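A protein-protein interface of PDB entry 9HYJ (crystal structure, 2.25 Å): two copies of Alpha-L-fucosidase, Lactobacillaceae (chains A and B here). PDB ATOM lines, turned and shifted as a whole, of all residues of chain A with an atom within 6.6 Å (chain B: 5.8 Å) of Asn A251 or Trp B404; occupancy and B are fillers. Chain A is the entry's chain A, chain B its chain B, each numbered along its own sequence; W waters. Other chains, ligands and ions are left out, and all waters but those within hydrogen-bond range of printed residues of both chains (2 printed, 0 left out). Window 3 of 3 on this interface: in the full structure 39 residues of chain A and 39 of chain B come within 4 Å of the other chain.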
ATOM      1  N   ALA A  29      38.308  21.281  14.876  1.00  0.00           N
ATOM      2  CA  ALA A  29      36.990  21.878  15.088  1.00  0.00           C
ATOM      3  C   ALA A  29      36.072  20.916  15.838  1.00  0.00           C
ATOM      4  O   ALA A  29      34.892  20.797  15.506  1.00  0.00           O
ATOM      5  CB  ALA A  29      36.372  22.315  13.754  1.00  0.00           C
ATOM      6  N   VAL A  30      36.627  20.226  16.840  1.00  0.00           N
ATOM      7  CA  VAL A  30      35.830  19.387  17.722  1.00  0.00           C
ATOM      8  C   VAL A  30      36.194  19.711  19.175  1.00  0.00           C
ATOM      9  O   VAL A  30      36.190  18.820  20.011  1.00  0.00           O
ATOM     10  CB  VAL A  30      35.939  17.865  17.429  1.00  0.00           C
ATOM     11  CG1 VAL A  30      35.265  17.442  16.112  1.00  0.00           C
ATOM     12  CG2 VAL A  30      37.383  17.385  17.427  1.00  0.00           C
ATOM     13  N   ASN A 243      28.674  28.743  22.250  1.00  0.00           N
ATOM     14  CA  ASN A 243      28.049  27.430  22.293  1.00  0.00           C
ATOM     15  C   ASN A 243      28.528  26.704  23.552  1.00  0.00           C
ATOM     16  O   ASN A 243      28.658  27.319  24.607  1.00  0.00           O
ATOM     17  CB  ASN A 243      28.146  26.721  20.940  1.00  0.00           C
ATOM     18  CG  ASN A 243      29.569  26.535  20.457  1.00  0.00           C
ATOM     19  OD1 ASN A 243      30.508  26.711  21.238  1.00  0.00           O
ATOM     20  ND2 ASN A 243      29.756  26.176  19.184  1.00  0.00           N
ATOM     21  N   ALA A 249      33.975  24.486  17.375  1.00  0.00           N
ATOM     22  CA  ALA A 249      33.354  23.164  17.365  1.00  0.00           C
ATOM     23  C   ALA A 249      32.237  23.171  16.316  1.00  0.00           C
ATOM     24  O   ALA A 249      31.124  23.625  16.590  1.00  0.00           O
ATOM     25  CB  ALA A 249      32.838  22.792  18.746  1.00  0.00           C
ATOM     26  N   ALA A 250      32.563  22.670  15.112  1.00  0.00           N
ATOM     27  CA  ALA A 250      31.752  22.889  13.926  1.00  0.00           C
ATOM     28  C   ALA A 250      30.357  22.281  14.091  1.00  0.00           C
ATOM     29  O   ALA A 250      29.402  22.827  13.563  1.00  0.00           O
ATOM     30  CB  ALA A 250      32.454  22.302  12.691  1.00  0.00           C
ATOM     31  N   ASN A 251      30.231  21.138  14.768  1.00  0.00           N
ATOM     32  CA  ASN A 251      28.918  20.517  14.933  1.00  0.00           C
ATOM     33  C   ASN A 251      28.373  20.733  16.345  1.00  0.00           C
ATOM     34  O   ASN A 251      27.576  19.933  16.860  1.00  0.00           O
ATOM     35  CB  ASN A 251      28.930  19.035  14.584  1.00  0.00           C
ATOM     36  CG  ASN A 251      29.104  18.828  13.095  1.00  0.00           C
ATOM     37  OD1 ASN A 251      28.517  19.541  12.255  1.00  0.00           O
ATOM     38  ND2 ASN A 251      29.940  17.858  12.780  1.00  0.00           N
ATOM     39  N   ASP A 252      28.825  21.801  16.997  1.00  0.00           N
ATOM     40  CA  ASP A 252      28.139  22.226  18.210  1.00  0.00           C
ATOM     41  C   ASP A 252      27.144  23.300  17.785  1.00  0.00           C
ATOM     42  O   ASP A 252      27.572  24.425  17.490  1.00  0.00           O
ATOM     43  CB  ASP A 252      29.125  22.701  19.275  1.00  0.00           C
ATOM     44  CG  ASP A 252      28.464  23.313  20.499  1.00  0.00           C
ATOM     45  OD1 ASP A 252      27.201  23.421  20.505  1.00  0.00           O
ATOM     46  OD2 ASP A 252      29.207  23.713  21.436  1.00  0.00           O
ATOM     47  N   LEU A 253      25.847  22.935  17.721  1.00  0.00           N
ATOM     48  CA  LEU A 253      24.809  23.836  17.217  1.00  0.00           C
ATOM     49  C   LEU A 253      24.116  24.519  18.388  1.00  0.00           C
ATOM     50  O   LEU A 253      23.177  25.307  18.197  1.00  0.00           O
ATOM     51  CB  LEU A 253      23.779  23.076  16.383  1.00  0.00           C
ATOM     52  CG  LEU A 253      24.343  22.131  15.313  1.00  0.00           C
ATOM     53  CD1 LEU A 253      23.203  21.527  14.522  1.00  0.00           C
ATOM     54  CD2 LEU A 253      25.358  22.849  14.411  1.00  0.00           C
ATOM     55  N   ASN A 254      24.560  24.186  19.601  1.00  0.00           N
ATOM     56  CA  ASN A 254      23.856  24.614  20.802  1.00  0.00           C
ATOM     57  C   ASN A 254      24.348  26.005  21.225  1.00  0.00           C
ATOM     58  O   ASN A 254      24.908  26.183  22.312  1.00  0.00           O
ATOM     59  CB  ASN A 254      23.969  23.517  21.859  1.00  0.00           C
ATOM     60  CG  ASN A 254      23.132  23.833  23.075  1.00  0.00           C
ATOM     61  OD1 ASN A 254      22.262  24.694  23.022  1.00  0.00           O
ATOM     62  ND2 ASN A 254      23.346  23.142  24.182  1.00  0.00           N
ATOM     63  N   ILE B 262      16.260  25.249  16.189  1.00  0.00           N
ATOM     64  CA  ILE B 262      16.282  23.821  15.915  1.00  0.00           C
ATOM     65  C   ILE B 262      15.123  23.128  16.639  1.00  0.00           C
ATOM     66  O   ILE B 262      14.441  22.291  16.054  1.00  0.00           O
ATOM     67  CB  ILE B 262      17.656  23.203  16.243  1.00  0.00           C
ATOM     68  CG1 ILE B 262      18.686  23.642  15.212  1.00  0.00           C
ATOM     69  CG2 ILE B 262      17.551  21.675  16.280  1.00  0.00           C
ATOM     70  CD1 ILE B 262      20.133  23.396  15.618  1.00  0.00           C
ATOM     71  N   ARG B 300      23.217  22.491   9.131  1.00  0.00           N
ATOM     72  CA  ARG B 300      23.928  21.315   9.621  1.00  0.00           C
ATOM     73  C   ARG B 300      22.920  20.373  10.274  1.00  0.00           C
ATOM     74  O   ARG B 300      23.025  19.158  10.125  1.00  0.00           O
ATOM     75  CB  ARG B 300      24.997  21.717  10.633  1.00  0.00           C
ATOM     76  CG  ARG B 300      26.185  22.369   9.944  1.00  0.00           C
ATOM     77  CD  ARG B 300      27.057  22.970  11.004  1.00  0.00           C
ATOM     78  NE  ARG B 300      28.309  23.472  10.454  1.00  0.00           N
ATOM     79  CZ  ARG B 300      29.339  22.694  10.097  1.00  0.00           C
ATOM     80  NH1 ARG B 300      29.343  21.391  10.321  1.00  0.00           N
ATOM     81  NH2 ARG B 300      30.387  23.241   9.498  1.00  0.00           N
ATOM     82  N   TRP B 301      21.925  20.923  10.981  1.00  0.00           N
ATOM     83  CA  TRP B 301      20.976  20.042  11.644  1.00  0.00           C
ATOM     84  C   TRP B 301      20.108  19.341  10.609  1.00  0.00           C
ATOM     85  O   TRP B 301      19.880  18.137  10.707  1.00  0.00           O
ATOM     86  CB  TRP B 301      20.109  20.823  12.642  1.00  0.00           C
ATOM     87  CG  TRP B 301      19.260  19.889  13.466  1.00  0.00           C
ATOM     88  CD1 TRP B 301      19.612  19.231  14.606  1.00  0.00           C
ATOM     89  CD2 TRP B 301      17.895  19.520  13.195  1.00  0.00           C
ATOM     90  NE1 TRP B 301      18.560  18.474  15.063  1.00  0.00           N
ATOM     91  CE2 TRP B 301      17.496  18.639  14.219  1.00  0.00           C
ATOM     92  CE3 TRP B 301      16.975  19.868  12.197  1.00  0.00           C
ATOM     93  CZ2 TRP B 301      16.215  18.069  14.265  1.00  0.00           C
ATOM     94  CZ3 TRP B 301      15.693  19.340  12.268  1.00  0.00           C
ATOM     95  CH2 TRP B 301      15.318  18.450  13.288  1.00  0.00           C
ATOM     96  N   MET B 304      21.693  16.433   8.882  1.00  0.00           N
ATOM     97  CA  MET B 304      21.736  15.248   9.725  1.00  0.00           C
ATOM     98  C   MET B 304      20.330  14.622   9.810  1.00  0.00           C
ATOM     99  O   MET B 304      20.211  13.398   9.839  1.00  0.00           O
ATOM    100  CB  MET B 304      22.318  15.624  11.098  1.00  0.00           C
ATOM    101  CG  MET B 304      22.241  14.544  12.183  1.00  0.00           C
ATOM    102  SD  MET B 304      20.577  14.300  12.858  1.00  0.00           S
ATOM    103  CE  MET B 304      20.315  15.799  13.830  1.00  0.00           C
ATOM    104  N   ASP B 375      23.590  10.948  13.809  1.00  0.00           N
ATOM    105  CA  ASP B 375      24.734  11.829  13.639  1.00  0.00           C
ATOM    106  C   ASP B 375      26.036  11.025  13.550  1.00  0.00           C
ATOM    107  O   ASP B 375      26.987  11.497  12.939  1.00  0.00           O
ATOM    108  CB  ASP B 375      24.817  12.856  14.753  1.00  0.00           C
ATOM    109  CG  ASP B 375      24.769  12.238  16.146  1.00  0.00           C
ATOM    110  OD1 ASP B 375      23.660  11.882  16.581  1.00  0.00           O
ATOM    111  OD2 ASP B 375      25.857  12.065  16.765  1.00  0.00           O
ATOM    112  N   TYR B 398      26.341  13.545  23.751  1.00  0.00           N
ATOM    113  CA  TYR B 398      27.059  13.892  22.538  1.00  0.00           C
ATOM    114  C   TYR B 398      28.547  13.588  22.696  1.00  0.00           C
ATOM    115  O   TYR B 398      29.142  13.841  23.744  1.00  0.00           O
ATOM    116  CB  TYR B 398      26.937  15.389  22.252  1.00  0.00           C
ATOM    117  CG  TYR B 398      25.487  15.792  22.063  1.00  0.00           C
ATOM    118  CD1 TYR B 398      24.789  15.349  20.946  1.00  0.00           C
ATOM    119  CD2 TYR B 398      24.822  16.603  22.997  1.00  0.00           C
ATOM    120  CE1 TYR B 398      23.455  15.684  20.771  1.00  0.00           C
ATOM    121  CE2 TYR B 398      23.491  16.969  22.821  1.00  0.00           C
ATOM    122  CZ  TYR B 398      22.824  16.504  21.701  1.00  0.00           C
ATOM    123  OH  TYR B 398      21.522  16.778  21.466  1.00  0.00           O
ATOM    124  N   GLY B 401      32.784  17.962  21.469  1.00  0.00           N
ATOM    125  CA  GLY B 401      32.971  18.728  20.252  1.00  0.00           C
ATOM    126  C   GLY B 401      31.703  18.821  19.412  1.00  0.00           C
ATOM    127  O   GLY B 401      31.698  19.478  18.377  1.00  0.00           O
ATOM    128  N   SER B 402      30.623  18.152  19.825  1.00  0.00           N
ATOM    129  CA  SER B 402      29.391  18.301  19.075  1.00  0.00           C
ATOM    130  C   SER B 402      28.192  18.453  20.023  1.00  0.00           C
ATOM    131  O   SER B 402      28.291  18.133  21.214  1.00  0.00           O
ATOM    132  CB  SER B 402      29.259  17.172  18.092  1.00  0.00           C
ATOM    133  OG  SER B 402      28.855  15.990  18.785  1.00  0.00           O
ATOM    134  N   ASP B 403      27.067  18.967  19.494  1.00  0.00           N
ATOM    135  CA  ASP B 403      25.834  19.141  20.253  1.00  0.00           C
ATOM    136  C   ASP B 403      24.719  19.482  19.258  1.00  0.00           C
ATOM    137  O   ASP B 403      24.687  20.574  18.700  1.00  0.00           O
ATOM    138  CB  ASP B 403      25.986  20.157  21.379  1.00  0.00           C
ATOM    139  CG  ASP B 403      24.764  20.320  22.286  1.00  0.00           C
ATOM    140  OD1 ASP B 403      23.633  20.013  21.824  1.00  0.00           O
ATOM    141  OD2 ASP B 403      24.929  20.745  23.464  1.00  0.00           O
ATOM    142  N   TRP B 404      23.827  18.518  19.026  1.00  0.00           N
ATOM    143  CA  TRP B 404      22.875  18.585  17.928  1.00  0.00           C
ATOM    144  C   TRP B 404      21.566  19.206  18.404  1.00  0.00           C
ATOM    145  O   TRP B 404      20.700  19.469  17.585  1.00  0.00           O
ATOM    146  CB  TRP B 404      22.655  17.195  17.317  1.00  0.00           C
ATOM    147  CG  TRP B 404      23.892  16.719  16.603  1.00  0.00           C
ATOM    148  CD1 TRP B 404      24.888  15.936  17.112  1.00  0.00           C
ATOM    149  CD2 TRP B 404      24.285  17.058  15.250  1.00  0.00           C
ATOM    150  NE1 TRP B 404      25.869  15.770  16.175  1.00  0.00           N
ATOM    151  CE2 TRP B 404      25.529  16.432  15.024  1.00  0.00           C
ATOM    152  CE3 TRP B 404      23.691  17.806  14.221  1.00  0.00           C
ATOM    153  CZ2 TRP B 404      26.195  16.528  13.803  1.00  0.00           C
ATOM    154  CZ3 TRP B 404      24.354  17.912  13.017  1.00  0.00           C
ATOM    155  CH2 TRP B 404      25.596  17.284  12.815  1.00  0.00           C
ATOM    156  N   VAL B 405      21.431  19.433  19.722  1.00  0.00           N
ATOM    157  CA  VAL B 405      20.252  20.070  20.313  1.00  0.00           C
ATOM    158  C   VAL B 405      19.070  19.100  20.298  1.00  0.00           C
ATOM    159  O   VAL B 405      18.481  18.855  21.340  1.00  0.00           O
ATOM    160  CB  VAL B 405      19.843  21.431  19.706  1.00  0.00           C
ATOM    161  CG1 VAL B 405      18.604  22.018  20.381  1.00  0.00           C
ATOM    162  CG2 VAL B 405      20.985  22.442  19.730  1.00  0.00           C
ATOM    163  N   VAL B 406      18.665  18.639  19.104  1.00  0.00           N
ATOM    164  CA  VAL B 406      17.697  17.569  18.992  1.00  0.00           C
ATOM    165  C   VAL B 406      18.404  16.405  18.295  1.00  0.00           C
ATOM    166  O   VAL B 406      18.735  16.495  17.104  1.00  0.00           O
ATOM    167  CB  VAL B 406      16.403  17.965  18.239  1.00  0.00           C
ATOM    168  CG1 VAL B 406      15.489  16.735  18.040  1.00  0.00           C
ATOM    169  CG2 VAL B 406      15.650  19.117  18.937  1.00  0.00           C
ATOM    170  N   ARG B 407      18.653  15.332  19.043  1.00  0.00           N
ATOM    171  CA  ARG B 407      19.368  14.174  18.535  1.00  0.00           C
ATOM    172  C   ARG B 407      18.335  13.147  18.085  1.00  0.00           C
ATOM    173  O   ARG B 407      17.277  13.013  18.706  1.00  0.00           O
ATOM    174  CB  ARG B 407      20.281  13.564  19.606  1.00  0.00           C
ATOM    175  CG  ARG B 407      21.532  12.967  18.953  1.00  0.00           C
ATOM    176  CD  ARG B 407      22.411  12.293  20.008  1.00  0.00           C
ATOM    177  NE  ARG B 407      23.632  11.824  19.351  1.00  0.00           N
ATOM    178  CZ  ARG B 407      24.657  11.293  19.990  1.00  0.00           C
ATOM    179  NH1 ARG B 407      24.611  11.111  21.308  1.00  0.00           N
ATOM    180  NH2 ARG B 407      25.737  10.957  19.301  1.00  0.00           N
HETATM  181  O   HOH W   1      32.354  19.450  15.803  1.00  0.00           O
HETATM  182  O   HOH W   2      27.470  18.740   9.858  1.00  0.00           O
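The backbone carbonyl oxygen (O) of Ala A250 lies within hydrogen-bond range of the guanidinium group (NE) of Arg B300, 3.4 Å away. The guanidinium group (NH1) of Arg B300 lies within hydrogen-bond range of the side-chain amide oxygen (OD1) of Asn A251 (2.8 Å). The backbone carbonyl oxygen (O) of Asn A251 is in hydrogen-bond range of the backbone NH (N) of Asp B403, 2.9 Å away. O of Asp B403 lies within hydrogen-bond range of N of Leu A253 (2.8 Å). OD2 of Asp B403 is in hydrogen-bond range of ND2 of Asn A254.
O of Ala A29 sits at hydrogen-bond distance from N of Ala A250. The backbone NH (N) of Asn A254 lies within hydrogen-bond range of the side-chain carboxylate (OD1) of Asp A252 (2.9 Å). The indole nitrogen of Trp B301 lies close to the backbone carbonyl oxygen of Trp B404, 3.5 Å away. The indole nitrogen of Trp B301 is in hydrogen-bond range of the backbone carbonyl oxygen of Val B406, 2.8 Å away. OH of Tyr B398 is in hydrogen-bond range of N of Val B405 (3.2 Å). The backbone NH (N) of Val B405 sits at hydrogen-bond distance from the side-chain carboxylate (OD1) of Asp B403 (3.1 Å).
O of Val A30 touches CA of Gly B401 (3.2 Å). Gly B401 touches Ala A249. OD1 of Asn A251 touches CH2 of Trp B404, at 3.7 Å. Asp A252 touches Gly B401 (N to O, 3.9 Å). CB of Asp B403 touches OD1 of Asp A252, at 3.6 Å. Ile B262 touches Leu A253. Leu A253 touches Arg B300. CD1 of Leu A253 touches CB of Trp B301 (3.7 Å). Trp B404 touches Leu A253 (CE3 to CD1, 3.8 Å). Val B405 touches Asn A254.
Printed residues of chain B within 4 Å of Val A30: Gly B401. Of the printed residues of chain B, Ala A249 touches Gly B401 (3.5 Å). Asn A251 touches just these residues of chain B: Arg B300 (2.8 Å), Ser B402 (3.3 Å), Asp B403 (2.9 Å) and Trp B404 (3.7 Å). Of the printed residues of chain A, Trp B301 touches Leu A253. Of the printed residues of chain A, Asp B403 touches Asn A251 (2.9 Å), Asp A252 (3.6 Å), Leu A253 (2.8 Å) and Asn A254 (3.0 Å). Trp B404 touches just these residues of chain A: Asn A251 and Leu A253. Printed residues of chain A within 4 Å of Val B405: Leu A253 (3.9 Å) and Asn A254 (3.8 Å).
Hydrophobic or aromatic side chains of chain B within 4 Å of the printed part of chain A: Ile B262, Trp B301, Trp B404 and Val B405. Of the 9 printed residues of chain A, 7 touch a printed residue of chain B. Printed residues of chain A that touch a printed residue of chain B: Val A30, Ala A249, Ala A250, Asn A251, Asp A252, Leu A253 and Asn A254. Among the printed residues, 17 pairs touch across the chains.
No position is printed for both chains. Of the 17 pairs that touch across the chains among the printed residues, none has its exchanged pair printed and touching as well.
Water W1 lies within hydrogen-bond range of the backbone carbonyl oxygen of Gly B401 (2.7 Å), the backbone carbonyl oxygen of Ala A29 (2.9 Å), the backbone NH of Asn A251 (2.9 Å) and the backbone NH of Ala A250 (3.3 Å). Water W2 lies within hydrogen-bond range of the side-chain amide oxygen of Asn A251 (2.7 Å) and the guanidinium group of Arg B300 (3.3 Å).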
